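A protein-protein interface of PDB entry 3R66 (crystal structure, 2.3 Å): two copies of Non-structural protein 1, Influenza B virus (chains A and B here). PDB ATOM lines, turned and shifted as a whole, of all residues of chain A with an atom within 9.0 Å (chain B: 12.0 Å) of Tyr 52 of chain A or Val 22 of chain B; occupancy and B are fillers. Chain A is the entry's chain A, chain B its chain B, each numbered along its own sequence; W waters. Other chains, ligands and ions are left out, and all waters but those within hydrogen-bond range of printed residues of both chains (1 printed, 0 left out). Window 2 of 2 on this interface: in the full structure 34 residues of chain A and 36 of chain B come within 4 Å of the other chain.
The backbone carbonyl oxygen (O) of Ala 49 of chain A lies within hydrogen-bond range of the side-chain hydroxyl (OG1) of Thr 30 of chain B.
O of Ala 26 of chain B sits close to O of Ala 49 of chain A (3.1 Å).
OE1 of Gln 55 of chain A lies close to N of Ile 20 of chain B, at 3.5 Å.
OH of Tyr 41 of chain A sits at hydrogen-bond distance from OE2 of Glu 34 of chain B, at 2.5 Å.
The backbone NH of Asp 51 of chain A lies within hydrogen-bond range of the side-chain hydroxyl of Thr 30 of chain B, at 2.9 Å.
O of Val 22 of chain B lies close to O of Arg 48 of chain A (3.2 Å).
NE of Arg 57 of chain A is in salt-bridge range of OE2 of Glu 34 of chain B (2.7 Å).
The backbone carbonyl oxygen (O) of Ala 26 of chain B sits at hydrogen-bond distance from the side-chain hydroxyl (OG1) of Thr 30 of chain B (2.9 Å).
O of Pro 53 of chain A sits at hydrogen-bond distance from NH1 of Arg 57 of chain A (3.3 Å).
The side-chain carboxylate of Glu 34 of chain B lies within salt-bridge range of the guanidinium group of Arg 68 of chain B (2.8 Å).
The backbone carbonyl oxygen (O) of Leu 50 of chain A is in hydrogen-bond range of the side-chain amide nitrogen (NE2) of Gln 55 of chain A (2.9 Å).
OD1 of Asp 51 of chain A sits at hydrogen-bond distance from N of Gly 54 of chain A (2.8 Å).
Among the printed residues, pairs that only touch across the chains: Tyr 41 of chain A with Phe 33 of chain B, Phe 44 of chain A with Ala 29 of chain B, Phe 44 of chain A with Thr 30 of chain B, Phe 44 of chain A with Phe 33 of chain B, Ser 45 of chain A with Ile 20 of chain B, Arg 48 of chain A with Glu 21 of chain B, Ala 49 of chain A with Ala 29 of chain B, Leu 50 of chain A with Val 22 of chain B, Leu 50 of chain A with Thr 30 of chain B, Asp 51 of chain A with Ala 26 of chain B, Asp 51 of chain A with Thr 27 of chain B, Tyr 52 of chain A with Val 22 of chain B, Gln 55 of chain A with Gln 19 of chain B, Gln 55 of chain A with Val 22 of chain B, Arg 57 of chain A with Lys 64 of chain B, Arg 57 of chain A with Arg 68 of chain B and His 59 of chain A with Thr 17 of chain B.
Leu 50 of chain A touches just these residues of chain B: Val 22 (3.0 Å) and Thr 30 (3.4 Å).
No residue of chain B comes within 4 Å of Pro 53 of chain A.
No residue of chain B comes within 4 Å of Gly 54 of chain A.
Gln 55 of chain A touches just these residues of chain B: Gln 19 (3.7 Å), Ile 20 (3.1 Å) and Val 22 (3.4 Å).
Of the printed residues of chain A, Ala 26 of chain B touches Ala 49 (3.1 Å) and Asp 51 (3.97 Å).
Of the printed residues of chain A, Thr 30 of chain B touches Phe 44 (3.9 Å), Ala 49 (2.8 Å), Leu 50 (3.4 Å) and Asp 51 (2.9 Å).
Ile 31 of chain B touches none of the printed residues of chain A.
The nearest residue of chain B that does not touch Tyr 52 of chain A is Glu 21 of chain B (4.1 Å).
The nearest printed residue of chain B that does not touch His 59 of chain A is Thr 18 of chain B (4.5 Å).
Hydrophobic or aromatic side chains of chain B within 4 Å of the printed part of chain A: Ile 20, Val 22, Ala 26, Ala 29 and Phe 33.
Hydrophobic or aromatic side chains of chain A that line the printed part of chain B: Tyr 41, Phe 44, Ala 49, Leu 50, Tyr 52 and His 59.
Among the printed residues, Asp or Glu carboxylates within 4 Å of a Lys or Arg side-chain nitrogen of the other chain: Arg 57 of chain A with Glu 34 of chain B.
No position is printed for both chains.
Of the 24 pairs that touch across the chains among the printed residues, none has its exchanged pair printed and touching as well.
Water W1 lies within hydrogen-bond range of OD2 of Asp 51 of chain A (2.7 Å), NH2 of Arg 68 of chain B (2.8 Å) and O of Thr 27 of chain B (2.9 Å).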
ATOM      1  N   TYR A  41     -29.090   6.446  -1.706  1.00  0.00           N
ATOM      2  CA  TYR A  41     -28.569   5.159  -1.193  1.00  0.00           C
ATOM      3  C   TYR A  41     -29.705   4.330  -0.644  1.00  0.00           C
ATOM      4  O   TYR A  41     -29.899   3.191  -1.048  1.00  0.00           O
ATOM      5  CB  TYR A  41     -27.469   5.345  -0.147  1.00  0.00           C
ATOM      6  CG  TYR A  41     -26.048   5.355  -0.707  1.00  0.00           C
ATOM      7  CD1 TYR A  41     -25.280   4.201  -0.761  1.00  0.00           C
ATOM      8  CD2 TYR A  41     -25.465   6.542  -1.137  1.00  0.00           C
ATOM      9  CE1 TYR A  41     -23.965   4.223  -1.241  1.00  0.00           C
ATOM     10  CE2 TYR A  41     -24.164   6.578  -1.640  1.00  0.00           C
ATOM     11  CZ  TYR A  41     -23.420   5.421  -1.700  1.00  0.00           C
ATOM     12  OH  TYR A  41     -22.126   5.486  -2.173  1.00  0.00           O
ATOM     13  N   PHE A  44     -32.136   3.175  -3.405  1.00  0.00           N
ATOM     14  CA  PHE A  44     -31.435   2.113  -4.125  1.00  0.00           C
ATOM     15  C   PHE A  44     -31.491   0.822  -3.307  1.00  0.00           C
ATOM     16  O   PHE A  44     -31.716  -0.260  -3.861  1.00  0.00           O
ATOM     17  CB  PHE A  44     -29.986   2.518  -4.391  1.00  0.00           C
ATOM     18  CG  PHE A  44     -29.230   1.591  -5.303  1.00  0.00           C
ATOM     19  CD1 PHE A  44     -29.674   1.344  -6.586  1.00  0.00           C
ATOM     20  CD2 PHE A  44     -28.041   0.996  -4.883  1.00  0.00           C
ATOM     21  CE1 PHE A  44     -28.980   0.510  -7.434  1.00  0.00           C
ATOM     22  CE2 PHE A  44     -27.332   0.155  -5.735  1.00  0.00           C
ATOM     23  CZ  PHE A  44     -27.804  -0.074  -7.014  1.00  0.00           C
ATOM     24  N   SER A  45     -31.311   0.930  -1.992  1.00  0.00           N
ATOM     25  CA  SER A  45     -31.232  -0.275  -1.154  1.00  0.00           C
ATOM     26  C   SER A  45     -32.540  -1.088  -1.219  1.00  0.00           C
ATOM     27  O   SER A  45     -32.518  -2.304  -1.100  1.00  0.00           O
ATOM     28  CB  SER A  45     -30.854   0.044   0.315  1.00  0.00           C
ATOM     29  OG  SER A  45     -31.929   0.608   1.041  1.00  0.00           O
ATOM     30  N   GLN A  47     -34.238  -1.619  -3.746  1.00  0.00           N
ATOM     31  CA  GLN A  47     -34.214  -2.368  -4.984  1.00  0.00           C
ATOM     32  C   GLN A  47     -33.365  -3.644  -4.866  1.00  0.00           C
ATOM     33  O   GLN A  47     -33.163  -4.329  -5.852  1.00  0.00           O
ATOM     34  CB  GLN A  47     -33.668  -1.475  -6.118  1.00  0.00           C
ATOM     35  CG  GLN A  47     -34.156  -0.023  -6.128  1.00  0.00           C
ATOM     36  CD  GLN A  47     -35.647   0.100  -5.927  1.00  0.00           C
ATOM     37  OE1 GLN A  47     -36.410  -0.673  -6.482  1.00  0.00           O
ATOM     38  NE2 GLN A  47     -36.068   1.076  -5.123  1.00  0.00           N
ATOM     39  N   ARG A  48     -32.861  -3.928  -3.675  1.00  0.00           N
ATOM     40  CA  ARG A  48     -32.012  -5.087  -3.441  1.00  0.00           C
ATOM     41  C   ARG A  48     -30.804  -5.121  -4.349  1.00  0.00           C
ATOM     42  O   ARG A  48     -30.367  -6.168  -4.779  1.00  0.00           O
ATOM     43  CB  ARG A  48     -32.802  -6.368  -3.617  1.00  0.00           C
ATOM     44  CG  ARG A  48     -33.785  -6.625  -2.518  1.00  0.00           C
ATOM     45  CD  ARG A  48     -35.171  -6.678  -3.061  1.00  0.00           C
ATOM     46  NE  ARG A  48     -36.159  -6.810  -2.010  1.00  0.00           N
ATOM     47  CZ  ARG A  48     -36.840  -7.918  -1.800  1.00  0.00           C
ATOM     48  NH1 ARG A  48     -37.738  -7.986  -0.830  1.00  0.00           N
ATOM     49  NH2 ARG A  48     -36.613  -8.959  -2.570  1.00  0.00           N
ATOM     50  N   ALA A  49     -30.273  -3.950  -4.628  1.00  0.00           N
ATOM     51  CA  ALA A  49     -29.148  -3.776  -5.530  1.00  0.00           C
ATOM     52  C   ALA A  49     -27.880  -3.344  -4.779  1.00  0.00           C
ATOM     53  O   ALA A  49     -26.781  -3.390  -5.337  1.00  0.00           O
ATOM     54  CB  ALA A  49     -29.505  -2.739  -6.591  1.00  0.00           C
ATOM     55  N   LEU A  50     -28.027  -2.928  -3.519  1.00  0.00           N
ATOM     56  CA  LEU A  50     -26.911  -2.380  -2.785  1.00  0.00           C
ATOM     57  C   LEU A  50     -26.143  -3.522  -2.118  1.00  0.00           C
ATOM     58  O   LEU A  50     -26.678  -4.176  -1.242  1.00  0.00           O
ATOM     59  CB  LEU A  50     -27.393  -1.348  -1.752  1.00  0.00           C
ATOM     60  CG  LEU A  50     -26.276  -0.532  -1.097  1.00  0.00           C
ATOM     61  CD1 LEU A  50     -25.555   0.245  -2.186  1.00  0.00           C
ATOM     62  CD2 LEU A  50     -26.837   0.426  -0.065  1.00  0.00           C
ATOM     63  N   ASP A  51     -24.910  -3.781  -2.559  1.00  0.00           N
ATOM     64  CA  ASP A  51     -24.105  -4.897  -2.025  1.00  0.00           C
ATOM     65  C   ASP A  51     -23.655  -4.614  -0.595  1.00  0.00           C
ATOM     66  O   ASP A  51     -23.894  -3.528  -0.079  1.00  0.00           O
ATOM     67  CB  ASP A  51     -22.906  -5.207  -2.938  1.00  0.00           C
ATOM     68  CG  ASP A  51     -21.860  -4.097  -2.964  1.00  0.00           C
ATOM     69  OD1 ASP A  51     -22.023  -3.087  -2.248  1.00  0.00           O
ATOM     70  OD2 ASP A  51     -20.862  -4.249  -3.711  1.00  0.00           O
ATOM     71  N   TYR A  52     -23.023  -5.583   0.057  1.00  0.00           N
ATOM     72  CA  TYR A  52     -22.780  -5.474   1.504  1.00  0.00           C
ATOM     73  C   TYR A  52     -21.822  -4.326   1.885  1.00  0.00           C
ATOM     74  O   TYR A  52     -22.161  -3.521   2.752  1.00  0.00           O
ATOM     75  CB  TYR A  52     -22.359  -6.829   2.105  1.00  0.00           C
ATOM     76  CG  TYR A  52     -23.434  -7.884   1.912  1.00  0.00           C
ATOM     77  CD1 TYR A  52     -24.696  -7.735   2.493  1.00  0.00           C
ATOM     78  CD2 TYR A  52     -23.203  -9.015   1.124  1.00  0.00           C
ATOM     79  CE1 TYR A  52     -25.696  -8.680   2.306  1.00  0.00           C
ATOM     80  CE2 TYR A  52     -24.198  -9.965   0.923  1.00  0.00           C
ATOM     81  CZ  TYR A  52     -25.444  -9.799   1.513  1.00  0.00           C
ATOM     82  OH  TYR A  52     -26.434 -10.743   1.317  1.00  0.00           O
ATOM     83  N   PRO A  53     -20.663  -4.208   1.214  1.00  0.00           N
ATOM     84  CA  PRO A  53     -19.830  -3.015   1.432  1.00  0.00           C
ATOM     85  C   PRO A  53     -20.566  -1.706   1.131  1.00  0.00           C
ATOM     86  O   PRO A  53     -20.346  -0.704   1.824  1.00  0.00           O
ATOM     87  CB  PRO A  53     -18.665  -3.198   0.445  1.00  0.00           C
ATOM     88  CG  PRO A  53     -18.651  -4.660   0.135  1.00  0.00           C
ATOM     89  CD  PRO A  53     -20.088  -5.098   0.192  1.00  0.00           C
ATOM     90  N   GLY A  54     -21.454  -1.726   0.131  1.00  0.00           N
ATOM     91  CA  GLY A  54     -22.262  -0.557  -0.213  1.00  0.00           C
ATOM     92  C   GLY A  54     -23.198  -0.163   0.920  1.00  0.00           C
ATOM     93  O   GLY A  54     -23.353   1.022   1.233  1.00  0.00           O
ATOM     94  N   GLN A  55     -23.813  -1.168   1.541  1.00  0.00           N
ATOM     95  CA  GLN A  55     -24.706  -0.937   2.660  1.00  0.00           C
ATOM     96  C   GLN A  55     -23.936  -0.386   3.869  1.00  0.00           C
ATOM     97  O   GLN A  55     -24.499   0.350   4.686  1.00  0.00           O
ATOM     98  CB  GLN A  55     -25.434  -2.217   3.040  1.00  0.00           C
ATOM     99  CG  GLN A  55     -26.559  -2.605   2.098  1.00  0.00           C
ATOM    100  CD  GLN A  55     -27.196  -3.949   2.462  1.00  0.00           C
ATOM    101  OE1 GLN A  55     -27.615  -4.170   3.610  1.00  0.00           O
ATOM    102  NE2 GLN A  55     -27.277  -4.851   1.484  1.00  0.00           N
ATOM    103  N   ASP A  56     -22.656  -0.736   3.982  1.00  0.00           N
ATOM    104  CA  ASP A  56     -21.832  -0.180   5.055  1.00  0.00           C
ATOM    105  C   ASP A  56     -21.553   1.292   4.812  1.00  0.00           C
ATOM    106  O   ASP A  56     -21.659   2.105   5.736  1.00  0.00           O
ATOM    107  CB  ASP A  56     -20.578  -1.013   5.328  1.00  0.00           C
ATOM    108  CG  ASP A  56     -20.624  -1.603   6.679  1.00  0.00           C
ATOM    109  OD1 ASP A  56     -20.219  -0.904   7.617  1.00  0.00           O
ATOM    110  OD2 ASP A  56     -21.133  -2.732   6.810  1.00  0.00           O
ATOM    111  N   ARG A  57     -21.280   1.645   3.559  1.00  0.00           N
ATOM    112  CA  ARG A  57     -21.150   3.045   3.179  1.00  0.00           C
ATOM    113  C   ARG A  57     -22.436   3.835   3.411  1.00  0.00           C
ATOM    114  O   ARG A  57     -22.359   4.983   3.833  1.00  0.00           O
ATOM    115  CB  ARG A  57     -20.665   3.192   1.727  1.00  0.00           C
ATOM    116  CG  ARG A  57     -19.206   2.759   1.548  1.00  0.00           C
ATOM    117  CD  ARG A  57     -18.638   3.114   0.175  1.00  0.00           C
ATOM    118  NE  ARG A  57     -19.195   2.302  -0.917  1.00  0.00           N
ATOM    119  CZ  ARG A  57     -18.895   1.020  -1.141  1.00  0.00           C
ATOM    120  NH1 ARG A  57     -18.051   0.350  -0.355  1.00  0.00           N
ATOM    121  NH2 ARG A  57     -19.469   0.388  -2.155  1.00  0.00           N
ATOM    122  N   LEU A  58     -23.603   3.231   3.152  1.00  0.00           N
ATOM    123  CA  LEU A  58     -24.909   3.845   3.494  1.00  0.00           C
ATOM    124  C   LEU A  58     -24.988   4.168   4.974  1.00  0.00           C
ATOM    125  O   LEU A  58     -25.174   5.326   5.337  1.00  0.00           O
ATOM    126  CB  LEU A  58     -26.106   2.938   3.115  1.00  0.00           C
ATOM    127  CG  LEU A  58     -27.518   3.538   3.299  1.00  0.00           C
ATOM    128  CD1 LEU A  58     -28.586   2.684   2.613  1.00  0.00           C
ATOM    129  CD2 LEU A  58     -27.880   3.789   4.765  1.00  0.00           C
ATOM    130  N   HIS A  59     -24.880   3.140   5.819  1.00  0.00           N
ATOM    131  CA  HIS A  59     -25.009   3.311   7.272  1.00  0.00           C
ATOM    132  C   HIS A  59     -23.963   4.243   7.826  1.00  0.00           C
ATOM    133  O   HIS A  59     -24.237   5.009   8.756  1.00  0.00           O
ATOM    134  CB  HIS A  59     -24.946   1.965   8.004  1.00  0.00           C
ATOM    135  CG  HIS A  59     -26.053   1.001   7.620  1.00  0.00           C
ATOM    136  ND1 HIS A  59     -27.359   1.322   7.708  1.00  0.00           N
ATOM    137  CD2 HIS A  59     -26.002  -0.311   7.147  1.00  0.00           C
ATOM    138  CE1 HIS A  59     -28.104   0.275   7.300  1.00  0.00           C
ATOM    139  NE2 HIS A  59     -27.273  -0.723   6.958  1.00  0.00           N
ATOM    140  N   ARG A  60     -22.763   4.207   7.256  1.00  0.00           N
ATOM    141  CA  ARG A  60     -21.709   5.107   7.677  1.00  0.00           C
ATOM    142  C   ARG A  60     -22.073   6.553   7.417  1.00  0.00           C
ATOM    143  O   ARG A  60     -21.911   7.401   8.289  1.00  0.00           O
ATOM    144  CB  ARG A  60     -20.432   4.790   6.916  1.00  0.00           C
ATOM    145  CG  ARG A  60     -19.381   5.882   7.025  1.00  0.00           C
ATOM    146  CD  ARG A  60     -18.036   5.457   6.480  1.00  0.00           C
ATOM    147  NE  ARG A  60     -17.061   6.536   6.633  1.00  0.00           N
ATOM    148  CZ  ARG A  60     -16.400   6.818   7.757  1.00  0.00           C
ATOM    149  NH1 ARG A  60     -16.593   6.116   8.874  1.00  0.00           N
ATOM    150  NH2 ARG A  60     -15.533   7.822   7.767  1.00  0.00           N
ATOM    151  N   THR B  17     -29.169  -2.075  13.078  1.00  0.00           N
ATOM    152  CA  THR B  17     -29.090  -2.003  11.592  1.00  0.00           C
ATOM    153  C   THR B  17     -29.801  -3.189  10.966  1.00  0.00           C
ATOM    154  O   THR B  17     -29.645  -4.318  11.427  1.00  0.00           O
ATOM    155  CB  THR B  17     -27.629  -2.004  11.111  1.00  0.00           C
ATOM    156  OG1 THR B  17     -26.995  -0.780  11.496  1.00  0.00           O
ATOM    157  CG2 THR B  17     -27.553  -2.155   9.603  1.00  0.00           C
ATOM    158  N   THR B  18     -30.580  -2.922   9.919  1.00  0.00           N
ATOM    159  CA  THR B  18     -31.315  -3.966   9.205  1.00  0.00           C
ATOM    160  C   THR B  18     -30.799  -4.168   7.767  1.00  0.00           C
ATOM    161  O   THR B  18     -30.922  -3.282   6.922  1.00  0.00           O
ATOM    162  CB  THR B  18     -32.836  -3.672   9.213  1.00  0.00           C
ATOM    163  OG1 THR B  18     -33.558  -4.841   8.798  1.00  0.00           O
ATOM    164  CG2 THR B  18     -33.197  -2.487   8.311  1.00  0.00           C
ATOM    165  N   GLN B  19     -30.212  -5.343   7.521  1.00  0.00           N
ATOM    166  CA  GLN B  19     -29.703  -5.740   6.199  1.00  0.00           C
ATOM    167  C   GLN B  19     -30.861  -6.068   5.255  1.00  0.00           C
ATOM    168  O   GLN B  19     -31.883  -6.612   5.682  1.00  0.00           O
ATOM    169  CB  GLN B  19     -28.754  -6.952   6.309  1.00  0.00           C
ATOM    170  CG  GLN B  19     -27.383  -6.654   6.938  1.00  0.00           C
ATOM    171  CD  GLN B  19     -27.406  -6.711   8.462  1.00  0.00           C
ATOM    172  OE1 GLN B  19     -27.944  -7.650   9.053  1.00  0.00           O
ATOM    173  NE2 GLN B  19     -26.807  -5.710   9.104  1.00  0.00           N
ATOM    174  N   ILE B  20     -30.690  -5.729   3.975  1.00  0.00           N
ATOM    175  CA  ILE B  20     -31.758  -5.849   2.987  1.00  0.00           C
ATOM    176  C   ILE B  20     -31.568  -7.046   2.038  1.00  0.00           C
ATOM    177  O   ILE B  20     -32.498  -7.396   1.310  1.00  0.00           O
ATOM    178  CB  ILE B  20     -31.889  -4.533   2.184  1.00  0.00           C
ATOM    179  CG1 ILE B  20     -31.776  -3.319   3.129  1.00  0.00           C
ATOM    180  CG2 ILE B  20     -33.208  -4.481   1.419  1.00  0.00           C
ATOM    181  CD1 ILE B  20     -30.381  -2.729   3.224  1.00  0.00           C
ATOM    182  N   GLU B  21     -30.386  -7.672   2.055  1.00  0.00           N
ATOM    183  CA  GLU B  21     -30.075  -8.861   1.231  1.00  0.00           C
ATOM    184  C   GLU B  21     -30.183  -8.513  -0.252  1.00  0.00           C
ATOM    185  O   GLU B  21     -31.003  -7.689  -0.638  1.00  0.00           O
ATOM    186  CB  GLU B  21     -30.966 -10.058   1.599  1.00  0.00           C
ATOM    187  CG  GLU B  21     -30.486 -11.396   1.036  1.00  0.00           C
ATOM    188  CD  GLU B  21     -31.348 -12.581   1.448  1.00  0.00           C
ATOM    189  OE1 GLU B  21     -32.450 -12.372   2.003  1.00  0.00           O
ATOM    190  OE2 GLU B  21     -30.925 -13.732   1.209  1.00  0.00           O
ATOM    191  N   VAL B  22     -29.349  -9.144  -1.074  1.00  0.00           N
ATOM    192  CA  VAL B  22     -28.982  -8.572  -2.370  1.00  0.00           C
ATOM    193  C   VAL B  22     -29.107  -9.532  -3.566  1.00  0.00           C
ATOM    194  O   VAL B  22     -29.935  -9.312  -4.472  1.00  0.00           O
ATOM    195  CB  VAL B  22     -27.553  -7.974  -2.256  1.00  0.00           C
ATOM    196  CG1 VAL B  22     -27.498  -7.022  -1.076  1.00  0.00           C
ATOM    197  CG2 VAL B  22     -26.494  -9.041  -2.053  1.00  0.00           C
ATOM    198  N   GLY B  23     -28.297 -10.594  -3.541  1.00  0.00           N
ATOM    199  CA  GLY B  23     -28.118 -11.524  -4.660  1.00  0.00           C
ATOM    200  C   GLY B  23     -26.928 -11.191  -5.564  1.00  0.00           C
ATOM    201  O   GLY B  23     -26.306 -10.122  -5.411  1.00  0.00           O
ATOM    202  N   PRO B  24     -26.588 -12.112  -6.503  1.00  0.00           N
ATOM    203  CA  PRO B  24     -25.534 -11.865  -7.502  1.00  0.00           C
ATOM    204  C   PRO B  24     -25.842 -10.592  -8.328  1.00  0.00           C
ATOM    205  O   PRO B  24     -27.021 -10.267  -8.562  1.00  0.00           O
ATOM    206  CB  PRO B  24     -25.527 -13.140  -8.380  1.00  0.00           C
ATOM    207  CG  PRO B  24     -26.581 -14.047  -7.844  1.00  0.00           C
ATOM    208  CD  PRO B  24     -27.144 -13.475  -6.580  1.00  0.00           C
ATOM    209  N   GLY B  25     -24.818  -9.847  -8.732  1.00  0.00           N
ATOM    210  CA  GLY B  25     -25.049  -8.654  -9.551  1.00  0.00           C
ATOM    211  C   GLY B  25     -25.484  -7.409  -8.796  1.00  0.00           C
ATOM    212  O   GLY B  25     -25.717  -6.376  -9.412  1.00  0.00           O
ATOM    213  N   ALA B  26     -25.631  -7.509  -7.476  1.00  0.00           N
ATOM    214  CA  ALA B  26     -25.611  -6.329  -6.617  1.00  0.00           C
ATOM    215  C   ALA B  26     -24.281  -5.601  -6.762  1.00  0.00           C
ATOM    216  O   ALA B  26     -24.227  -4.366  -6.706  1.00  0.00           O
ATOM    217  CB  ALA B  26     -25.814  -6.723  -5.171  1.00  0.00           C
ATOM    218  N   THR B  27     -23.216  -6.382  -6.932  1.00  0.00           N
ATOM    219  CA  THR B  27     -21.881  -5.847  -7.051  1.00  0.00           C
ATOM    220  C   THR B  27     -21.776  -4.898  -8.250  1.00  0.00           C
ATOM    221  O   THR B  27     -21.370  -3.747  -8.099  1.00  0.00           O
ATOM    222  CB  THR B  27     -20.844  -6.989  -7.172  1.00  0.00           C
ATOM    223  OG1 THR B  27     -21.163  -7.809  -8.303  1.00  0.00           O
ATOM    224  CG2 THR B  27     -20.835  -7.876  -5.907  1.00  0.00           C
ATOM    225  N   ASN B  28     -22.172  -5.359  -9.429  1.00  0.00           N
ATOM    226  CA  ASN B  28     -22.171  -4.510 -10.617  1.00  0.00           C
ATOM    227  C   ASN B  28     -23.129  -3.318 -10.494  1.00  0.00           C
ATOM    228  O   ASN B  28     -22.768  -2.184 -10.816  1.00  0.00           O
ATOM    229  CB  ASN B  28     -22.511  -5.312 -11.870  1.00  0.00           C
ATOM    230  CG  ASN B  28     -22.248  -4.522 -13.129  1.00  0.00           C
ATOM    231  OD1 ASN B  28     -21.113  -4.139 -13.409  1.00  0.00           O
ATOM    232  ND2 ASN B  28     -23.301  -4.245 -13.881  1.00  0.00           N
ATOM    233  N   ALA B  29     -24.346  -3.584 -10.028  1.00  0.00           N
ATOM    234  CA  ALA B  29     -25.351  -2.538  -9.790  1.00  0.00           C
ATOM    235  C   ALA B  29     -24.839  -1.432  -8.864  1.00  0.00           C
ATOM    236  O   ALA B  29     -25.045  -0.241  -9.148  1.00  0.00           O
ATOM    237  CB  ALA B  29     -26.624  -3.141  -9.222  1.00  0.00           C
ATOM    238  N   THR B  30     -24.165  -1.813  -7.774  1.00  0.00           N
ATOM    239  CA  THR B  30     -23.616  -0.826  -6.837  1.00  0.00           C
ATOM    240  C   THR B  30     -22.481   0.007  -7.480  1.00  0.00           C
ATOM    241  O   THR B  30     -22.418   1.216  -7.278  1.00  0.00           O
ATOM    242  CB  THR B  30     -23.158  -1.475  -5.516  1.00  0.00           C
ATOM    243  OG1 THR B  30     -24.284  -2.108  -4.876  1.00  0.00           O
ATOM    244  CG2 THR B  30     -22.606  -0.426  -4.560  1.00  0.00           C
ATOM    245  N   ILE B  31     -21.626  -0.613  -8.286  1.00  0.00           N
ATOM    246  CA  ILE B  31     -20.562   0.145  -8.964  1.00  0.00           C
ATOM    247  C   ILE B  31     -21.163   1.213  -9.867  1.00  0.00           C
ATOM    248  O   ILE B  31     -20.679   2.348  -9.915  1.00  0.00           O
ATOM    249  CB  ILE B  31     -19.641  -0.761  -9.829  1.00  0.00           C
ATOM    250  CG1 ILE B  31     -18.787  -1.685  -8.954  1.00  0.00           C
ATOM    251  CG2 ILE B  31     -18.749   0.091 -10.710  1.00  0.00           C
ATOM    252  CD1 ILE B  31     -18.083  -2.803  -9.713  1.00  0.00           C
ATOM    253  N   PHE B  33     -24.426   2.501  -9.797  1.00  0.00           N
ATOM    254  CA  PHE B  33     -25.051   3.478  -8.904  1.00  0.00           C
ATOM    255  C   PHE B  33     -24.006   4.419  -8.319  1.00  0.00           C
ATOM    256  O   PHE B  33     -24.151   5.629  -8.383  1.00  0.00           O
ATOM    257  CB  PHE B  33     -25.777   2.761  -7.765  1.00  0.00           C
ATOM    258  CG  PHE B  33     -26.345   3.677  -6.723  1.00  0.00           C
ATOM    259  CD1 PHE B  33     -27.495   4.402  -6.978  1.00  0.00           C
ATOM    260  CD2 PHE B  33     -25.747   3.803  -5.480  1.00  0.00           C
ATOM    261  CE1 PHE B  33     -28.038   5.237  -6.015  1.00  0.00           C
ATOM    262  CE2 PHE B  33     -26.286   4.635  -4.501  1.00  0.00           C
ATOM    263  CZ  PHE B  33     -27.434   5.348  -4.770  1.00  0.00           C
ATOM    264  N   GLU B  34     -22.950   3.861  -7.744  1.00  0.00           N
ATOM    265  CA  GLU B  34     -21.965   4.713  -7.084  1.00  0.00           C
ATOM    266  C   GLU B  34     -21.144   5.539  -8.064  1.00  0.00           C
ATOM    267  O   GLU B  34     -20.664   6.613  -7.713  1.00  0.00           O
ATOM    268  CB  GLU B  34     -21.086   3.899  -6.162  1.00  0.00           C
ATOM    269  CG  GLU B  34     -21.804   3.658  -4.846  1.00  0.00           C
ATOM    270  CD  GLU B  34     -20.947   2.961  -3.834  1.00  0.00           C
ATOM    271  OE1 GLU B  34     -20.249   2.005  -4.212  1.00  0.00           O
ATOM    272  OE2 GLU B  34     -20.988   3.356  -2.665  1.00  0.00           O
ATOM    273  N   LYS B  64     -11.404   4.824  -5.231  1.00  0.00           N
ATOM    274  CA  LYS B  64     -11.932   3.496  -4.875  1.00  0.00           C
ATOM    275  C   LYS B  64     -12.716   2.869  -6.033  1.00  0.00           C
ATOM    276  O   LYS B  64     -12.580   1.682  -6.322  1.00  0.00           O
ATOM    277  CB  LYS B  64     -12.863   3.579  -3.659  1.00  0.00           C
ATOM    278  CG  LYS B  64     -12.219   3.949  -2.330  1.00  0.00           C
ATOM    279  CD  LYS B  64     -13.263   3.994  -1.201  1.00  0.00           C
ATOM    280  CE  LYS B  64     -14.192   5.216  -1.280  1.00  0.00           C
ATOM    281  NZ  LYS B  64     -15.585   4.925  -0.819  1.00  0.00           N
ATOM    282  N   ARG B  68     -12.172  -0.506  -8.173  1.00  0.00           N
ATOM    283  CA  ARG B  68     -13.262  -1.495  -8.173  1.00  0.00           C
ATOM    284  C   ARG B  68     -13.717  -1.842  -9.604  1.00  0.00           C
ATOM    285  O   ARG B  68     -14.027  -3.000  -9.893  1.00  0.00           O
ATOM    286  CB  ARG B  68     -14.455  -0.984  -7.343  1.00  0.00           C
ATOM    287  CG  ARG B  68     -14.382  -1.138  -5.819  1.00  0.00           C
ATOM    288  CD  ARG B  68     -15.379  -0.186  -5.156  1.00  0.00           C
ATOM    289  NE  ARG B  68     -16.771  -0.580  -5.397  1.00  0.00           N
ATOM    290  CZ  ARG B  68     -17.811   0.252  -5.444  1.00  0.00           C
ATOM    291  NH1 ARG B  68     -17.660   1.568  -5.285  1.00  0.00           N
ATOM    292  NH2 ARG B  68     -19.027  -0.239  -5.681  1.00  0.00           N
HETATM  293  O   HOH W   1     -19.848  -2.895  -5.773  1.00  0.00           O
